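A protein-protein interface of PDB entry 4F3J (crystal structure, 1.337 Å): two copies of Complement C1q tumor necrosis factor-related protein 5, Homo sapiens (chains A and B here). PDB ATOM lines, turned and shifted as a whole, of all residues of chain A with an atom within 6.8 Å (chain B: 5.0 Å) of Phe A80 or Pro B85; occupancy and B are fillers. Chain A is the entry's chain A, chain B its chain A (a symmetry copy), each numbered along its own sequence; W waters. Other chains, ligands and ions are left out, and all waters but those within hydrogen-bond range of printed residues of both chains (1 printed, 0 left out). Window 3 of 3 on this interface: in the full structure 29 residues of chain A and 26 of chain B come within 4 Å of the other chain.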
ATOM      1  N   VAL A  58      33.785 -15.933  15.783  1.00  0.00           N
ATOM      2  CA  VAL A  58      33.390 -16.507  14.503  1.00  0.00           C
ATOM      3  C   VAL A  58      34.624 -16.607  13.606  1.00  0.00           C
ATOM      4  O   VAL A  58      35.331 -15.618  13.404  1.00  0.00           O
ATOM      5  CB  VAL A  58      32.320 -15.609  13.811  1.00  0.00           C
ATOM      6  CG1 VAL A  58      31.892 -16.219  12.475  1.00  0.00           C
ATOM      7  CG2 VAL A  58      31.105 -15.394  14.745  1.00  0.00           C
ATOM      8  N   ALA A  61      34.047 -19.721   8.816  1.00  0.00           N
ATOM      9  CA  ALA A  61      32.726 -20.051   8.316  1.00  0.00           C
ATOM     10  C   ALA A  61      31.831 -19.115   9.071  1.00  0.00           C
ATOM     11  O   ALA A  61      32.143 -18.732  10.211  1.00  0.00           O
ATOM     12  CB  ALA A  61      32.273 -21.490   8.554  1.00  0.00           C
ATOM     13  N   SER A  62      30.700 -18.756   8.475  1.00  0.00           N
ATOM     14  CA  SER A  62      29.686 -17.992   9.200  1.00  0.00           C
ATOM     15  C   SER A  62      29.162 -18.778  10.398  1.00  0.00           C
ATOM     16  O   SER A  62      29.323 -20.011  10.468  1.00  0.00           O
ATOM     17  CB  SER A  62      28.521 -17.620   8.275  1.00  0.00           C
ATOM     18  OG  SER A  62      28.957 -16.817   7.190  1.00  0.00           O
ATOM     19  N   LEU A  63      28.551 -18.074  11.348  1.00  0.00           N
ATOM     20  CA  LEU A  63      27.970 -18.718  12.520  1.00  0.00           C
ATOM     21  C   LEU A  63      26.513 -18.351  12.668  1.00  0.00           C
ATOM     22  O   LEU A  63      26.158 -17.165  12.697  1.00  0.00           O
ATOM     23  CB  LEU A  63      28.715 -18.327  13.800  1.00  0.00           C
ATOM     24  CG  LEU A  63      28.161 -18.883  15.116  1.00  0.00           C
ATOM     25  CD1 LEU A  63      28.174 -20.412  15.090  1.00  0.00           C
ATOM     26  CD2 LEU A  63      28.946 -18.338  16.321  1.00  0.00           C
ATOM     27  N   PHE A  78      23.016 -14.593  13.959  1.00  0.00           N
ATOM     28  CA  PHE A  78      23.860 -14.916  12.821  1.00  0.00           C
ATOM     29  C   PHE A  78      24.901 -13.831  12.562  1.00  0.00           C
ATOM     30  O   PHE A  78      24.610 -12.642  12.645  1.00  0.00           O
ATOM     31  CB  PHE A  78      23.000 -15.098  11.565  1.00  0.00           C
ATOM     32  CG  PHE A  78      23.792 -15.457  10.339  1.00  0.00           C
ATOM     33  CD1 PHE A  78      24.083 -16.782  10.062  1.00  0.00           C
ATOM     34  CD2 PHE A  78      24.261 -14.471   9.472  1.00  0.00           C
ATOM     35  CE1 PHE A  78      24.811 -17.117   8.929  1.00  0.00           C
ATOM     36  CE2 PHE A  78      24.990 -14.804   8.336  1.00  0.00           C
ATOM     37  CZ  PHE A  78      25.267 -16.130   8.072  1.00  0.00           C
ATOM     38  N   GLN A  79      26.103 -14.255  12.215  1.00  0.00           N
ATOM     39  CA  GLN A  79      27.132 -13.333  11.739  1.00  0.00           C
ATOM     40  C   GLN A  79      27.804 -13.924  10.495  1.00  0.00           C
ATOM     41  O   GLN A  79      28.334 -15.043  10.549  1.00  0.00           O
ATOM     42  CB  GLN A  79      28.199 -13.071  12.817  1.00  0.00           C
ATOM     43  CG  GLN A  79      29.431 -12.290  12.308  1.00  0.00           C
ATOM     44  CD  GLN A  79      29.096 -10.882  11.857  1.00  0.00           C
ATOM     45  OE1 GLN A  79      28.501 -10.092  12.581  1.00  0.00           O
ATOM     46  NE2 GLN A  79      29.501 -10.560  10.638  1.00  0.00           N
ATOM     47  N   PHE A  80      27.789 -13.188   9.375  1.00  0.00           N
ATOM     48  CA  PHE A  80      28.488 -13.566   8.151  1.00  0.00           C
ATOM     49  C   PHE A  80      29.993 -13.565   8.370  1.00  0.00           C
ATOM     50  O   PHE A  80      30.530 -12.651   8.982  1.00  0.00           O
ATOM     51  CB  PHE A  80      28.127 -12.557   7.071  1.00  0.00           C
ATOM     52  CG  PHE A  80      28.765 -12.839   5.747  1.00  0.00           C
ATOM     53  CD1 PHE A  80      28.483 -14.019   5.072  1.00  0.00           C
ATOM     54  CD2 PHE A  80      29.660 -11.937   5.173  1.00  0.00           C
ATOM     55  CE1 PHE A  80      29.071 -14.293   3.852  1.00  0.00           C
ATOM     56  CE2 PHE A  80      30.245 -12.185   3.928  1.00  0.00           C
ATOM     57  CZ  PHE A  80      29.959 -13.375   3.267  1.00  0.00           C
ATOM     58  N   PHE A  81      30.680 -14.595   7.876  1.00  0.00           N
ATOM     59  CA  PHE A  81      32.134 -14.562   7.869  1.00  0.00           C
ATOM     60  C   PHE A  81      32.602 -14.429   6.432  1.00  0.00           C
ATOM     61  O   PHE A  81      32.542 -15.389   5.652  1.00  0.00           O
ATOM     62  CB  PHE A  81      32.761 -15.809   8.499  1.00  0.00           C
ATOM     63  CG  PHE A  81      34.246 -15.688   8.691  1.00  0.00           C
ATOM     64  CD1 PHE A  81      34.727 -14.943   9.746  1.00  0.00           C
ATOM     65  CD2 PHE A  81      35.149 -16.256   7.801  1.00  0.00           C
ATOM     66  CE1 PHE A  81      36.081 -14.773   9.956  1.00  0.00           C
ATOM     67  CE2 PHE A  81      36.515 -16.108   8.012  1.00  0.00           C
ATOM     68  CZ  PHE A  81      36.971 -15.355   9.104  1.00  0.00           C
ATOM     69  N   GLY A  82      33.088 -13.239   6.081  1.00  0.00           N
ATOM     70  CA  GLY A  82      33.461 -12.901   4.715  1.00  0.00           C
ATOM     71  C   GLY A  82      34.836 -13.349   4.248  1.00  0.00           C
ATOM     72  O   GLY A  82      35.476 -12.662   3.443  1.00  0.00           O
ATOM     73  N   GLY A  83      35.301 -14.496   4.740  1.00  0.00           N
ATOM     74  CA  GLY A  83      36.558 -15.059   4.256  1.00  0.00           C
ATOM     75  C   GLY A  83      37.787 -14.321   4.774  1.00  0.00           C
ATOM     76  O   GLY A  83      38.892 -14.492   4.248  1.00  0.00           O
ATOM     77  N   TRP A  84      37.596 -13.518   5.815  1.00  0.00           N
ATOM     78  CA  TRP A  84      38.641 -12.669   6.382  1.00  0.00           C
ATOM     79  C   TRP A  84      39.792 -13.498   6.967  1.00  0.00           C
ATOM     80  O   TRP A  84      39.619 -14.689   7.269  1.00  0.00           O
ATOM     81  CB  TRP A  84      38.019 -11.752   7.456  1.00  0.00           C
ATOM     82  CG  TRP A  84      36.871 -10.946   6.911  1.00  0.00           C
ATOM     83  CD1 TRP A  84      36.892 -10.143   5.804  1.00  0.00           C
ATOM     84  CD2 TRP A  84      35.526 -10.889   7.418  1.00  0.00           C
ATOM     85  NE1 TRP A  84      35.653  -9.575   5.600  1.00  0.00           N
ATOM     86  CE2 TRP A  84      34.798 -10.016   6.573  1.00  0.00           C
ATOM     87  CE3 TRP A  84      34.873 -11.468   8.519  1.00  0.00           C
ATOM     88  CZ2 TRP A  84      33.452  -9.713   6.790  1.00  0.00           C
ATOM     89  CZ3 TRP A  84      33.536 -11.169   8.726  1.00  0.00           C
ATOM     90  CH2 TRP A  84      32.840 -10.298   7.867  1.00  0.00           C
ATOM     91  N   ALA A  88      35.807 -12.862  13.385  1.00  0.00           N
ATOM     92  CA  ALA A  88      34.761 -11.883  13.665  1.00  0.00           C
ATOM     93  C   ALA A  88      34.051 -12.283  14.971  1.00  0.00           C
ATOM     94  O   ALA A  88      34.529 -13.161  15.706  1.00  0.00           O
ATOM     95  CB  ALA A  88      33.777 -11.836  12.503  1.00  0.00           C
ATOM     96  N   SER A  89      32.929 -11.637  15.288  1.00  0.00           N
ATOM     97  CA  SER A  89      32.255 -11.864  16.548  1.00  0.00           C
ATOM     98  C   SER A  89      30.741 -11.799  16.385  1.00  0.00           C
ATOM     99  O   SER A  89      30.217 -11.159  15.457  1.00  0.00           O
ATOM    100  CB  SER A  89      32.711 -10.811  17.537  1.00  0.00           C
ATOM    101  OG  SER A  89      32.157  -9.547  17.218  1.00  0.00           O
ATOM    102  N   TYR A 113      26.655 -23.299   8.859  1.00  0.00           N
ATOM    103  CA  TYR A 113      27.074 -22.122   9.602  1.00  0.00           C
ATOM    104  C   TYR A 113      27.560 -22.430  11.026  1.00  0.00           C
ATOM    105  O   TYR A 113      26.965 -22.022  12.026  1.00  0.00           O
ATOM    106  CB  TYR A 113      25.967 -21.062   9.556  1.00  0.00           C
ATOM    107  CG  TYR A 113      25.592 -20.667   8.135  1.00  0.00           C
ATOM    108  CD1 TYR A 113      26.559 -20.575   7.128  1.00  0.00           C
ATOM    109  CD2 TYR A 113      24.276 -20.369   7.801  1.00  0.00           C
ATOM    110  CE1 TYR A 113      26.212 -20.211   5.849  1.00  0.00           C
ATOM    111  CE2 TYR A 113      23.925 -20.009   6.524  1.00  0.00           C
ATOM    112  CZ  TYR A 113      24.893 -19.927   5.558  1.00  0.00           C
ATOM    113  OH  TYR A 113      24.532 -19.569   4.290  1.00  0.00           O
ATOM    114  N   TYR B  59      21.314  -6.119   8.216  1.00  0.00           N
ATOM    115  CA  TYR B  59      21.226  -6.653   6.860  1.00  0.00           C
ATOM    116  C   TYR B  59      20.784  -5.591   5.879  1.00  0.00           C
ATOM    117  O   TYR B  59      19.852  -4.842   6.158  1.00  0.00           O
ATOM    118  CB  TYR B  59      20.187  -7.775   6.838  1.00  0.00           C
ATOM    119  CG  TYR B  59      20.112  -8.625   5.569  1.00  0.00           C
ATOM    120  CD1 TYR B  59      21.257  -9.110   4.933  1.00  0.00           C
ATOM    121  CD2 TYR B  59      18.875  -9.028   5.085  1.00  0.00           C
ATOM    122  CE1 TYR B  59      21.154  -9.926   3.782  1.00  0.00           C
ATOM    123  CE2 TYR B  59      18.760  -9.835   3.973  1.00  0.00           C
ATOM    124  CZ  TYR B  59      19.890 -10.288   3.332  1.00  0.00           C
ATOM    125  OH  TYR B  59      19.720 -11.105   2.258  1.00  0.00           O
ATOM    126  N   GLY B  83      27.869  -4.657   2.321  1.00  0.00           N
ATOM    127  CA  GLY B  83      27.270  -5.144   1.082  1.00  0.00           C
ATOM    128  C   GLY B  83      27.289  -6.663   0.960  1.00  0.00           C
ATOM    129  O   GLY B  83      27.081  -7.210  -0.127  1.00  0.00           O
ATOM    130  N   TRP B  84      27.521  -7.339   2.080  1.00  0.00           N
ATOM    131  CA  TRP B  84      27.662  -8.793   2.130  1.00  0.00           C
ATOM    132  C   TRP B  84      26.365  -9.505   1.720  1.00  0.00           C
ATOM    133  O   TRP B  84      25.279  -8.906   1.762  1.00  0.00           O
ATOM    134  CB  TRP B  84      28.095  -9.209   3.551  1.00  0.00           C
ATOM    135  CG  TRP B  84      29.352  -8.505   3.986  1.00  0.00           C
ATOM    136  CD1 TRP B  84      30.539  -8.466   3.308  1.00  0.00           C
ATOM    137  CD2 TRP B  84      29.542  -7.710   5.169  1.00  0.00           C
ATOM    138  NE1 TRP B  84      31.463  -7.713   4.001  1.00  0.00           N
ATOM    139  CE2 TRP B  84      30.877  -7.237   5.144  1.00  0.00           C
ATOM    140  CE3 TRP B  84      28.726  -7.373   6.261  1.00  0.00           C
ATOM    141  CZ2 TRP B  84      31.411  -6.444   6.162  1.00  0.00           C
ATOM    142  CZ3 TRP B  84      29.257  -6.582   7.265  1.00  0.00           C
ATOM    143  CH2 TRP B  84      30.588  -6.127   7.210  1.00  0.00           C
ATOM    144  N   PRO B  85      26.468 -10.787   1.317  1.00  0.00           N
ATOM    145  CA  PRO B  85      25.265 -11.525   0.906  1.00  0.00           C
ATOM    146  C   PRO B  85      24.367 -11.945   2.074  1.00  0.00           C
ATOM    147  O   PRO B  85      23.197 -12.237   1.856  1.00  0.00           O
ATOM    148  CB  PRO B  85      25.835 -12.767   0.204  1.00  0.00           C
ATOM    149  CG  PRO B  85      27.178 -12.956   0.799  1.00  0.00           C
ATOM    150  CD  PRO B  85      27.694 -11.578   1.113  1.00  0.00           C
ATOM    151  N   LYS B  86      24.907 -11.988   3.288  1.00  0.00           N
ATOM    152  CA  LYS B  86      24.148 -12.460   4.446  1.00  0.00           C
ATOM    153  C   LYS B  86      24.346 -11.508   5.609  1.00  0.00           C
ATOM    154  O   LYS B  86      25.253 -10.664   5.545  1.00  0.00           O
ATOM    155  CB  LYS B  86      24.566 -13.884   4.769  1.00  0.00           C
ATOM    156  CG  LYS B  86      24.187 -14.822   3.633  1.00  0.00           C
ATOM    157  CD  LYS B  86      24.505 -16.253   3.906  1.00  0.00           C
ATOM    158  CE  LYS B  86      24.319 -17.041   2.618  1.00  0.00           C
ATOM    159  NZ  LYS B  86      22.921 -16.927   2.076  1.00  0.00           N
ATOM    160  N   PRO B  87      23.498 -11.616   6.659  1.00  0.00           N
ATOM    161  CA  PRO B  87      23.538 -10.582   7.706  1.00  0.00           C
ATOM    162  C   PRO B  87      24.793 -10.555   8.569  1.00  0.00           C
ATOM    163  O   PRO B  87      25.550 -11.538   8.685  1.00  0.00           O
ATOM    164  CB  PRO B  87      22.335 -10.922   8.594  1.00  0.00           C
ATOM    165  CG  PRO B  87      21.429 -11.697   7.721  1.00  0.00           C
ATOM    166  CD  PRO B  87      22.332 -12.511   6.842  1.00  0.00           C
ATOM    167  N   ALA B  88      24.993  -9.391   9.175  1.00  0.00           N
ATOM    168  CA  ALA B  88      25.974  -9.188  10.236  1.00  0.00           C
ATOM    169  C   ALA B  88      25.225  -8.980  11.565  1.00  0.00           C
ATOM    170  O   ALA B  88      24.009  -9.214  11.647  1.00  0.00           O
ATOM    171  CB  ALA B  88      26.845  -7.982   9.908  1.00  0.00           C
HETATM  172  O   HOH W   1      34.664  -7.254   3.521  1.00  0.00           O
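N of Phe A80 lies within hydrogen-bond range of O of Pro B87 (2.9 Å).
Hydrophobic or aromatic side chains of chain A within 4 Å of the printed part of chain B: Phe A78, Phe A80, Trp A84 and Tyr A113. Printed residues of chain B that touch a printed residue of chain A: Trp B84, Pro B85, Lys B86, Pro B87 and Ala B88. Hydrophobic or aromatic side chains of chain B within 4 Å of the printed part of chain A: Trp B84, Pro B85, Pro B87 and Ala B88. Among the printed residues, no Asp or Glu carboxylate lies within 4 Å of a Lys or Arg side-chain nitrogen of the other chain.
Phe A80 touches just these residues of chain B: Trp B84 (3.5 Å), Pro B85 (3.6 Å), Lys B86 (3.8 Å) and Pro B87 (2.9 Å). Printed residues of chain B within 4 Å of Phe A78: Lys B86 (3.7 Å), Pro B87 (3.3 Å) and Ala B88 (3.6 Å). Of the printed residues of chain A, Ala B88 touches Phe A78 (3.6 Å) and Gln A79 (3.6 Å). Ala A61 touches none of the printed residues of chain B. Ala A88 touches none of the printed residues of chain B. The nearest printed residue of chain B that does not touch Phe A78 is Pro B85 (6.9 Å).
Trp B84 touches its own counterpart, Trp A84. Of the 11 pairs that touch across the chains among the printed residues, 1 has its exchanged pair printed and touching as well.
Water W1 lies within hydrogen-bond range of the indole nitrogen of Trp A84 (3.3 Å) and the indole nitrogen of Trp B84 (3.3 Å).
N of Gln A79 lies within hydrogen-bond range of O of Leu A63 (3.0 Å).
Among the printed residues, merely in contact across the chains: Tyr A113 with Lys B86 (3.0 Å), Phe A78 with Pro B87 (3.3 Å), Phe A80 with Trp B84 (3.5 Å), Gln A79 with Ala B88 (3.6 Å), Phe A80 with Pro B85 (3.6 Å), Phe A78 with Ala B88 (3.6 Å), Phe A78 with Lys B86 (3.7 Å), Gln A79 with Pro B87 (3.7 Å), Phe A80 with Lys B86 (3.8 Å) and Trp A84 with Trp B84 (3.9 Å).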
